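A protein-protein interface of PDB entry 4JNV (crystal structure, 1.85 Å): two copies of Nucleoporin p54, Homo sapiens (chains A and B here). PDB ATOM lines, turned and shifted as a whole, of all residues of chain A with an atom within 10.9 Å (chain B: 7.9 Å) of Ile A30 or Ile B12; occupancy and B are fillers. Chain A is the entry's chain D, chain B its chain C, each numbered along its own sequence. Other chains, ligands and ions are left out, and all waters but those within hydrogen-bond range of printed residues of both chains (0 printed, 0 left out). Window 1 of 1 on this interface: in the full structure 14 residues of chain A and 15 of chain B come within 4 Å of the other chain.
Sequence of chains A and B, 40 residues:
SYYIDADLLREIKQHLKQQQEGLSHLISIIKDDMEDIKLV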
ATOM      1  N   GLY A  22     -25.078  28.361  26.985  1.00  0.00           N
ATOM      2  CA  GLY A  22     -24.785  28.635  25.593  1.00  0.00           C
ATOM      3  C   GLY A  22     -25.515  27.659  24.691  1.00  0.00           C
ATOM      4  O   GLY A  22     -26.211  28.066  23.766  1.00  0.00           O
ATOM      5  N   LEU A  23     -25.371  26.369  24.973  1.00  0.00           N
ATOM      6  CA  LEU A  23     -25.995  25.340  24.156  1.00  0.00           C
ATOM      7  C   LEU A  23     -27.505  25.471  24.202  1.00  0.00           C
ATOM      8  O   LEU A  23     -28.190  25.240  23.202  1.00  0.00           O
ATOM      9  CB  LEU A  23     -25.590  23.949  24.634  1.00  0.00           C
ATOM     10  CG  LEU A  23     -24.092  23.673  24.650  1.00  0.00           C
ATOM     11  CD1 LEU A  23     -23.806  22.268  25.177  1.00  0.00           C
ATOM     12  CD2 LEU A  23     -23.516  23.863  23.259  1.00  0.00           C
ATOM     13  N   SER A  24     -28.030  25.851  25.363  1.00  0.00           N
ATOM     14  CA  SER A  24     -29.476  26.000  25.518  1.00  0.00           C
ATOM     15  C   SER A  24     -30.018  27.014  24.525  1.00  0.00           C
ATOM     16  O   SER A  24     -31.020  26.760  23.857  1.00  0.00           O
ATOM     17  CB  SER A  24     -29.837  26.412  26.943  1.00  0.00           C
ATOM     18  OG  SER A  24     -29.448  25.411  27.868  1.00  0.00           O
ATOM     19  N   HIS A  25     -29.357  28.163  24.426  1.00  0.00           N
ATOM     20  CA  HIS A  25     -29.728  29.161  23.429  1.00  0.00           C
ATOM     21  C   HIS A  25     -29.671  28.492  22.067  1.00  0.00           C
ATOM     22  O   HIS A  25     -30.667  28.419  21.350  1.00  0.00           O
ATOM     23  CB  HIS A  25     -28.768  30.355  23.472  1.00  0.00           C
ATOM     24  CG  HIS A  25     -29.439  31.682  23.280  1.00  0.00           C
ATOM     25  ND1 HIS A  25     -28.735  32.866  23.202  1.00  0.00           N
ATOM     26  CD2 HIS A  25     -30.746  32.017  23.163  1.00  0.00           C
ATOM     27  CE1 HIS A  25     -29.580  33.870  23.041  1.00  0.00           C
ATOM     28  NE2 HIS A  25     -30.807  33.381  23.014  1.00  0.00           N
ATOM     29  N   LEU A  26     -28.487  27.992  21.734  1.00  0.00           N
ATOM     30  CA  LEU A  26     -28.258  27.272  20.495  1.00  0.00           C
ATOM     31  C   LEU A  26     -29.454  26.388  20.170  1.00  0.00           C
ATOM     32  O   LEU A  26     -30.026  26.476  19.080  1.00  0.00           O
ATOM     33  CB  LEU A  26     -27.003  26.413  20.639  1.00  0.00           C
ATOM     34  CG  LEU A  26     -26.099  26.190  19.431  1.00  0.00           C
ATOM     35  CD1 LEU A  26     -25.747  27.497  18.751  1.00  0.00           C
ATOM     36  CD2 LEU A  26     -24.830  25.492  19.891  1.00  0.00           C
ATOM     37  N   ILE A  27     -29.835  25.544  21.121  1.00  0.00           N
ATOM     38  CA  ILE A  27     -30.893  24.574  20.874  1.00  0.00           C
ATOM     39  C   ILE A  27     -32.241  25.262  20.691  1.00  0.00           C
ATOM     40  O   ILE A  27     -33.016  24.898  19.809  1.00  0.00           O
ATOM     41  CB  ILE A  27     -30.987  23.539  22.001  1.00  0.00           C
ATOM     42  CG1 ILE A  27     -29.966  22.428  21.758  1.00  0.00           C
ATOM     43  CG2 ILE A  27     -32.394  22.967  22.072  1.00  0.00           C
ATOM     44  CD1 ILE A  27     -29.889  21.406  22.861  1.00  0.00           C
ATOM     45  N   SER A  28     -32.509  26.260  21.526  1.00  0.00           N
ATOM     46  CA  SER A  28     -33.749  27.013  21.448  1.00  0.00           C
ATOM     47  C   SER A  28     -33.935  27.675  20.087  1.00  0.00           C
ATOM     48  O   SER A  28     -35.022  27.631  19.506  1.00  0.00           O
ATOM     49  CB  SER A  28     -33.773  28.076  22.539  1.00  0.00           C
ATOM     50  OG  SER A  28     -33.886  27.473  23.810  1.00  0.00           O
ATOM     51  N   ILE A  29     -32.873  28.297  19.586  1.00  0.00           N
ATOM     52  CA  ILE A  29     -32.916  28.969  18.295  1.00  0.00           C
ATOM     53  C   ILE A  29     -33.116  27.961  17.170  1.00  0.00           C
ATOM     54  O   ILE A  29     -33.817  28.235  16.197  1.00  0.00           O
ATOM     55  CB  ILE A  29     -31.632  29.785  18.048  1.00  0.00           C
ATOM     56  CG1 ILE A  29     -31.696  31.115  18.795  1.00  0.00           C
ATOM     57  CG2 ILE A  29     -31.470  30.075  16.579  1.00  0.00           C
ATOM     58  CD1 ILE A  29     -31.763  30.986  20.293  1.00  0.00           C
ATOM     59  N   ILE A  30     -32.499  26.792  17.291  1.00  0.00           N
ATOM     60  CA  ILE A  30     -32.696  25.765  16.292  1.00  0.00           C
ATOM     61  C   ILE A  30     -34.165  25.318  16.311  1.00  0.00           C
ATOM     62  O   ILE A  30     -34.800  25.226  15.265  1.00  0.00           O
ATOM     63  CB  ILE A  30     -31.769  24.567  16.499  1.00  0.00           C
ATOM     64  CG1 ILE A  30     -30.313  24.970  16.254  1.00  0.00           C
ATOM     65  CG2 ILE A  30     -32.143  23.429  15.562  1.00  0.00           C
ATOM     66  CD1 ILE A  30     -29.349  23.934  16.684  1.00  0.00           C
ATOM     67  N   LYS A  31     -34.705  25.061  17.497  1.00  0.00           N
ATOM     68  CA  LYS A  31     -36.099  24.623  17.614  1.00  0.00           C
ATOM     69  C   LYS A  31     -37.069  25.580  16.934  1.00  0.00           C
ATOM     70  O   LYS A  31     -38.019  25.144  16.288  1.00  0.00           O
ATOM     71  CB  LYS A  31     -36.487  24.463  19.081  1.00  0.00           C
ATOM     72  CG  LYS A  31     -35.976  23.171  19.709  1.00  0.00           C
ATOM     73  CD  LYS A  31     -36.104  23.197  21.232  1.00  0.00           C
ATOM     74  CE  LYS A  31     -35.583  21.908  21.869  1.00  0.00           C
ATOM     75  NZ  LYS A  31     -35.424  22.005  23.354  1.00  0.00           N
ATOM     76  N   ASP A  32     -36.839  26.881  17.076  1.00  0.00           N
ATOM     77  CA  ASP A  32     -37.740  27.856  16.481  1.00  0.00           C
ATOM     78  C   ASP A  32     -37.647  27.802  14.961  1.00  0.00           C
ATOM     79  O   ASP A  32     -38.660  27.924  14.267  1.00  0.00           O
ATOM     80  CB  ASP A  32     -37.463  29.267  17.024  1.00  0.00           C
ATOM     81  CG  ASP A  32     -36.188  29.872  16.480  1.00  0.00           C
ATOM     82  OD1 ASP A  32     -35.779  29.509  15.361  1.00  0.00           O
ATOM     83  OD2 ASP A  32     -35.602  30.730  17.173  1.00  0.00           O
ATOM     84  N   ASP A  33     -36.445  27.600  14.433  1.00  0.00           N
ATOM     85  CA  ASP A  33     -36.283  27.515  12.987  1.00  0.00           C
ATOM     86  C   ASP A  33     -36.890  26.234  12.435  1.00  0.00           C
ATOM     87  O   ASP A  33     -37.375  26.200  11.304  1.00  0.00           O
ATOM     88  CB  ASP A  33     -34.812  27.625  12.593  1.00  0.00           C
ATOM     89  CG  ASP A  33     -34.362  29.066  12.442  1.00  0.00           C
ATOM     90  OD1 ASP A  33     -35.005  29.951  13.041  1.00  0.00           O
ATOM     91  OD2 ASP A  33     -33.370  29.317  11.722  1.00  0.00           O
ATOM     92  N   MET A  34     -36.885  25.174  13.230  1.00  0.00           N
ATOM     93  CA  MET A  34     -37.447  23.921  12.752  1.00  0.00           C
ATOM     94  C   MET A  34     -38.984  23.905  12.792  1.00  0.00           C
ATOM     95  O   MET A  34     -39.623  22.900  12.477  1.00  0.00           O
ATOM     96  CB  MET A  34     -36.814  22.762  13.502  1.00  0.00           C
ATOM     97  CG  MET A  34     -35.325  22.683  13.205  1.00  0.00           C
ATOM     98  SD  MET A  34     -34.546  21.028  13.812  1.00  0.00           S
ATOM     99  CE  MET A  34     -35.677  20.812  15.364  1.00  0.00           C
ATOM    100  N   GLU A  35     -39.570  25.047  13.133  1.00  0.00           N
ATOM    101  CA  GLU A  35     -41.006  25.230  13.045  1.00  0.00           C
ATOM    102  C   GLU A  35     -41.321  26.022  11.763  1.00  0.00           C
ATOM    103  O   GLU A  35     -42.452  26.429  11.531  1.00  0.00           O
ATOM    104  CB  GLU A  35     -41.526  25.936  14.299  1.00  0.00           C
ATOM    105  CG  GLU A  35     -41.043  25.262  15.584  1.00  0.00           C
ATOM    106  CD  GLU A  35     -41.491  25.976  16.843  1.00  0.00           C
ATOM    107  OE1 GLU A  35     -40.831  25.802  17.892  1.00  0.00           O
ATOM    108  OE2 GLU A  35     -42.505  26.701  16.792  1.00  0.00           O
ATOM    109  N   ASP A  36     -40.300  26.202  10.929  1.00  0.00           N
ATOM    110  CA  ASP A  36     -40.414  27.021   9.728  1.00  0.00           C
ATOM    111  C   ASP A  36     -39.787  26.304   8.533  1.00  0.00           C
ATOM    112  O   ASP A  36     -39.064  26.903   7.738  1.00  0.00           O
ATOM    113  CB  ASP A  36     -39.721  28.372   9.932  1.00  0.00           C
ATOM    114  CG  ASP A  36     -39.898  29.285   8.747  1.00  0.00           C
ATOM    115  OD1 ASP A  36     -40.901  29.096   8.027  1.00  0.00           O
ATOM    116  OD2 ASP A  36     -39.050  30.181   8.533  1.00  0.00           O
ATOM    117  N   ILE A  37     -40.070  25.014   8.423  1.00  0.00           N
ATOM    118  CA  ILE A  37     -39.477  24.174   7.411  1.00  0.00           C
ATOM    119  C   ILE A  37     -40.256  24.343   6.109  1.00  0.00           C
ATOM    120  O   ILE A  37     -41.476  24.565   6.133  1.00  0.00           O
ATOM    121  CB  ILE A  37     -39.559  22.717   7.866  1.00  0.00           C
ATOM    122  CG1 ILE A  37     -38.709  22.491   9.112  1.00  0.00           C
ATOM    123  CG2 ILE A  37     -39.138  21.775   6.778  1.00  0.00           C
ATOM    124  CD1 ILE A  37     -37.377  23.158   9.039  1.00  0.00           C
ATOM    125  N   ILE B   4     -34.554  24.014   5.433  1.00  0.00           N
ATOM    126  CA  ILE B   4     -34.580  25.139   6.350  1.00  0.00           C
ATOM    127  C   ILE B   4     -33.586  26.240   5.900  1.00  0.00           C
ATOM    128  O   ILE B   4     -32.590  25.920   5.237  1.00  0.00           O
ATOM    129  CB  ILE B   4     -34.206  24.663   7.762  1.00  0.00           C
ATOM    130  CG1 ILE B   4     -34.337  25.796   8.778  1.00  0.00           C
ATOM    131  CG2 ILE B   4     -32.804  24.132   7.765  1.00  0.00           C
ATOM    132  CD1 ILE B   4     -35.721  26.364   8.884  1.00  0.00           C
ATOM    133  N   ALA B   6     -30.663  28.597   5.515  1.00  0.00           N
ATOM    134  CA  ALA B   6     -29.266  28.210   5.704  1.00  0.00           C
ATOM    135  C   ALA B   6     -28.539  29.156   6.625  1.00  0.00           C
ATOM    136  O   ALA B   6     -27.476  28.819   7.151  1.00  0.00           O
ATOM    137  CB  ALA B   6     -28.558  28.158   4.356  1.00  0.00           C
ATOM    138  N   ASP B   7     -29.108  30.329   6.838  1.00  0.00           N
ATOM    139  CA  ASP B   7     -28.474  31.317   7.694  1.00  0.00           C
ATOM    140  C   ASP B   7     -28.173  30.761   9.079  1.00  0.00           C
ATOM    141  O   ASP B   7     -27.259  31.228   9.753  1.00  0.00           O
ATOM    142  CB  ASP B   7     -29.350  32.567   7.801  1.00  0.00           C
ATOM    143  CG  ASP B   7     -29.280  33.434   6.554  1.00  0.00           C
ATOM    144  OD1 ASP B   7     -28.282  33.330   5.807  1.00  0.00           O
ATOM    145  OD2 ASP B   7     -30.219  34.225   6.321  1.00  0.00           O
ATOM    146  N   LEU B   8     -28.938  29.759   9.496  1.00  0.00           N
ATOM    147  CA  LEU B   8     -28.779  29.179  10.820  1.00  0.00           C
ATOM    148  C   LEU B   8     -27.442  28.459  10.993  1.00  0.00           C
ATOM    149  O   LEU B   8     -26.945  28.350  12.106  1.00  0.00           O
ATOM    150  CB  LEU B   8     -29.920  28.206  11.105  1.00  0.00           C
ATOM    151  CG  LEU B   8     -30.028  27.758  12.562  1.00  0.00           C
ATOM    152  CD1 LEU B   8     -30.317  28.932  13.492  1.00  0.00           C
ATOM    153  CD2 LEU B   8     -31.089  26.702  12.697  1.00  0.00           C
ATOM    154  N   LEU B   9     -26.877  27.942   9.907  1.00  0.00           N
ATOM    155  CA  LEU B   9     -25.569  27.303   9.987  1.00  0.00           C
ATOM    156  C   LEU B   9     -24.520  28.310  10.448  1.00  0.00           C
ATOM    157  O   LEU B   9     -23.653  28.014  11.283  1.00  0.00           O
ATOM    158  CB  LEU B   9     -25.197  26.717   8.636  1.00  0.00           C
ATOM    159  CG  LEU B   9     -25.910  25.427   8.257  1.00  0.00           C
ATOM    160  CD1 LEU B   9     -25.659  25.119   6.800  1.00  0.00           C
ATOM    161  CD2 LEU B   9     -25.454  24.263   9.138  1.00  0.00           C
ATOM    162  N   ARG B  10     -24.622  29.516   9.914  1.00  0.00           N
ATOM    163  CA  ARG B  10     -23.745  30.615  10.281  1.00  0.00           C
ATOM    164  C   ARG B  10     -23.776  30.856  11.790  1.00  0.00           C
ATOM    165  O   ARG B  10     -22.735  30.921  12.452  1.00  0.00           O
ATOM    166  CB  ARG B  10     -24.210  31.871   9.545  1.00  0.00           C
ATOM    167  CG  ARG B  10     -23.293  33.074   9.657  1.00  0.00           C
ATOM    168  CD  ARG B  10     -24.108  34.360   9.672  1.00  0.00           C
ATOM    169  NE  ARG B  10     -24.889  34.470  10.905  1.00  0.00           N
ATOM    170  CZ  ARG B  10     -26.137  34.926  10.984  1.00  0.00           C
ATOM    171  NH1 ARG B  10     -26.788  35.330   9.899  1.00  0.00           N
ATOM    172  NH2 ARG B  10     -26.740  34.977  12.162  1.00  0.00           N
ATOM    173  N   GLU B  11     -24.981  30.992  12.333  1.00  0.00           N
ATOM    174  CA  GLU B  11     -25.147  31.328  13.738  1.00  0.00           C
ATOM    175  C   GLU B  11     -24.569  30.225  14.627  1.00  0.00           C
ATOM    176  O   GLU B  11     -23.788  30.485  15.545  1.00  0.00           O
ATOM    177  CB  GLU B  11     -26.632  31.545  14.036  1.00  0.00           C
ATOM    178  CG  GLU B  11     -26.911  32.115  15.415  1.00  0.00           C
ATOM    179  CD  GLU B  11     -28.251  32.830  15.498  1.00  0.00           C
ATOM    180  OE1 GLU B  11     -28.605  33.547  14.541  1.00  0.00           O
ATOM    181  OE2 GLU B  11     -28.951  32.675  16.522  1.00  0.00           O
ATOM    182  N   ILE B  12     -24.947  28.991  14.326  1.00  0.00           N
ATOM    183  CA  ILE B  12     -24.488  27.846  15.083  1.00  0.00           C
ATOM    184  C   ILE B  12     -22.973  27.752  15.093  1.00  0.00           C
ATOM    185  O   ILE B  12     -22.373  27.485  16.139  1.00  0.00           O
ATOM    186  CB  ILE B  12     -25.064  26.539  14.515  1.00  0.00           C
ATOM    187  CG1 ILE B  12     -26.587  26.511  14.675  1.00  0.00           C
ATOM    188  CG2 ILE B  12     -24.473  25.334  15.233  1.00  0.00           C
ATOM    189  CD1 ILE B  12     -27.252  25.367  13.918  1.00  0.00           C
ATOM    190  N   LYS B  13     -22.352  27.938  13.936  1.00  0.00           N
ATOM    191  CA  LYS B  13     -20.900  27.826  13.846  1.00  0.00           C
ATOM    192  C   LYS B  13     -20.260  28.890  14.710  1.00  0.00           C
ATOM    193  O   LYS B  13     -19.353  28.604  15.495  1.00  0.00           O
ATOM    194  CB  LYS B  13     -20.432  27.981  12.402  1.00  0.00           C
ATOM    195  CG  LYS B  13     -18.969  27.602  12.191  1.00  0.00           C
ATOM    196  CD  LYS B  13     -18.228  28.670  11.405  1.00  0.00           C
ATOM    197  CE  LYS B  13     -17.659  28.113  10.114  1.00  0.00           C
ATOM    198  NZ  LYS B  13     -16.587  27.109  10.349  1.00  0.00           N
ATOM    199  N   GLN B  14     -20.733  30.123  14.577  1.00  0.00           N
ATOM    200  CA  GLN B  14     -20.186  31.224  15.360  1.00  0.00           C
ATOM    201  C   GLN B  14     -20.141  30.886  16.848  1.00  0.00           C
ATOM    202  O   GLN B  14     -19.109  31.060  17.500  1.00  0.00           O
ATOM    203  CB  GLN B  14     -21.005  32.498  15.141  1.00  0.00           C
ATOM    204  CG  GLN B  14     -20.653  33.247  13.866  1.00  0.00           C
ATOM    205  CD  GLN B  14     -21.392  34.566  13.744  1.00  0.00           C
ATOM    206  OE1 GLN B  14     -22.432  34.769  14.370  1.00  0.00           O
ATOM    207  NE2 GLN B  14     -20.850  35.475  12.944  1.00  0.00           N
ATOM    208  N   HIS B  15     -21.256  30.398  17.383  1.00  0.00           N
ATOM    209  CA  HIS B  15     -21.350  30.113  18.812  1.00  0.00           C
ATOM    210  C   HIS B  15     -20.459  28.946  19.229  1.00  0.00           C
ATOM    211  O   HIS B  15     -19.820  28.982  20.289  1.00  0.00           O
ATOM    212  CB  HIS B  15     -22.804  29.831  19.209  1.00  0.00           C
ATOM    213  CG  HIS B  15     -23.611  31.071  19.443  1.00  0.00           C
ATOM    214  ND1 HIS B  15     -24.900  31.044  19.935  1.00  0.00           N
ATOM    215  CD2 HIS B  15     -23.310  32.378  19.254  1.00  0.00           C
ATOM    216  CE1 HIS B  15     -25.358  32.280  20.036  1.00  0.00           C
ATOM    217  NE2 HIS B  15     -24.411  33.108  19.630  1.00  0.00           N
ATOM    218  N   LEU B  16     -20.428  27.909  18.401  1.00  0.00           N
ATOM    219  CA  LEU B  16     -19.625  26.734  18.694  1.00  0.00           C
ATOM    220  C   LEU B  16     -18.150  27.093  18.732  1.00  0.00           C
ATOM    221  O   LEU B  16     -17.387  26.505  19.490  1.00  0.00           O
ATOM    222  CB  LEU B  16     -19.877  25.637  17.656  1.00  0.00           C
ATOM    223  CG  LEU B  16     -21.259  24.982  17.688  1.00  0.00           C
ATOM    224  CD1 LEU B  16     -21.301  23.840  16.687  1.00  0.00           C
ATOM    225  CD2 LEU B  16     -21.616  24.497  19.084  1.00  0.00           C
ATOM    226  N   LYS B  17     -17.753  28.047  17.898  1.00  0.00           N
ATOM    227  CA  LYS B  17     -16.385  28.563  17.909  1.00  0.00           C
ATOM    228  C   LYS B  17     -16.033  29.155  19.264  1.00  0.00           C
ATOM    229  O   LYS B  17     -14.919  28.966  19.764  1.00  0.00           O
ATOM    230  CB  LYS B  17     -16.204  29.644  16.839  1.00  0.00           C
ATOM    231  CG  LYS B  17     -16.068  29.114  15.440  1.00  0.00           C
ATOM    232  CD  LYS B  17     -14.788  28.325  15.275  1.00  0.00           C
ATOM    233  CE  LYS B  17     -15.052  27.034  14.536  1.00  0.00           C
ATOM    234  NZ  LYS B  17     -15.640  27.287  13.190  1.00  0.00           N
ATOM    235  N   GLN B  18     -16.977  29.893  19.841  1.00  0.00           N
ATOM    236  CA  GLN B  18     -16.787  30.484  21.160  1.00  0.00           C
ATOM    237  C   GLN B  18     -16.765  29.411  22.235  1.00  0.00           C
ATOM    238  O   GLN B  18     -15.837  29.339  23.047  1.00  0.00           O
ATOM    239  CB  GLN B  18     -17.893  31.497  21.477  1.00  0.00           C
ATOM    240  CG  GLN B  18     -18.417  31.393  22.912  1.00  0.00           C
ATOM    241  CD  GLN B  18     -19.068  32.673  23.422  1.00  0.00           C
ATOM    242  OE1 GLN B  18     -18.552  33.772  23.216  1.00  0.00           O
ATOM    243  NE2 GLN B  18     -20.200  32.528  24.110  1.00  0.00           N
ATOM    244  N   GLN B  19     -17.808  28.590  22.253  1.00  0.00           N
ATOM    245  CA  GLN B  19     -17.907  27.513  23.221  1.00  0.00           C
ATOM    246  C   GLN B  19     -16.644  26.659  23.153  1.00  0.00           C
ATOM    247  O   GLN B  19     -16.222  26.069  24.150  1.00  0.00           O
ATOM    248  CB  GLN B  19     -19.167  26.690  22.963  1.00  0.00           C
ATOM    249  CG  GLN B  19     -19.295  25.456  23.821  1.00  0.00           C
ATOM    250  CD  GLN B  19     -20.638  25.361  24.522  1.00  0.00           C
ATOM    251  OE1 GLN B  19     -21.458  26.282  24.460  1.00  0.00           O
ATOM    252  NE2 GLN B  19     -20.863  24.248  25.206  1.00  0.00           N
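Ile B12 touches Leu A26 (CA to CD1, 3.9 Å).
Leu A26 touches His B15 (CD1 to CB, 3.8 Å).
Leu B16 touches Leu A26 (CD2 to CD2, 3.5 Å).
Ile A29 touches Leu B8 (CG2 to CD1, 3.5 Å).
Ile A29 touches Glu B11 (CG2 to OE2, 3.6 Å).
Ile A30 touches Ile B12 (CD1 to CD1, 3.8 Å).
Asp A33 touches Ile B4.
Asp A33 touches Leu B8 (OD2 to CD1, 3.5 Å).
Asp A36 touches Ile B4.
CD1 of Ile A37 touches CD1 of Ile B4, at 3.6 Å.
Of chain A, only Leu A26 and Ile A30 come within 4 Å of Ile B12.
His B15 touches just one residue of chain A: Leu A26 (3.8 Å).
Leu B16 touches just one residue of chain A: Leu A26 (3.5 Å).
Of the printed residues of chain B, Asp A33 touches Ile B4 and Leu B8.
Printed residues of chain A within 4 Å of Ile B4: Asp A33, Asp A36 and Ile A37.
Printed residues of chain B within 4 Å of Leu A23: Gln B19 (3.3 Å).
Of the printed residues of chain A, Gln B19 touches Leu A23 (3.3 Å).
Arg B10 touches none of the printed residues of chain A.
The nearest printed residue of chain B that does not touch Leu A23 is Leu B16 (4.6 Å).
No position is printed for both chains.
Of the 11 pairs that touch across the chains among the printed residues, none has its exchanged pair printed and touching as well.
The side-chain carboxylate (OE1) of Glu B11 lies within salt-bridge range of the guanidinium group (NH2) of Arg B10 (3.3 Å).
The backbone carbonyl oxygen of Ile A29 sits close to the side-chain carboxylate of Asp A32, 2.5 Å away.
The side-chain carboxylate (OD1) of Asp A33 sits close to the side-chain carboxylate (OD1) of Asp A32, 2.5 Å away.
Printed residues of chain B that touch a printed residue of chain A: Ile B4, Leu B8, Glu B11, Ile B12, His B15, Leu B16 and Gln B19.
Hydrophobic or aromatic side chains of chain B within 4 Å of the printed part of chain A: Ile B4, Leu B8, Ile B12, His B15 and Leu B16.
Printed residues of chain A that touch a printed residue of chain B: Leu A23, Leu A26, Ile A29, Ile A30, Asp A33, Asp A36 and Ile A37.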
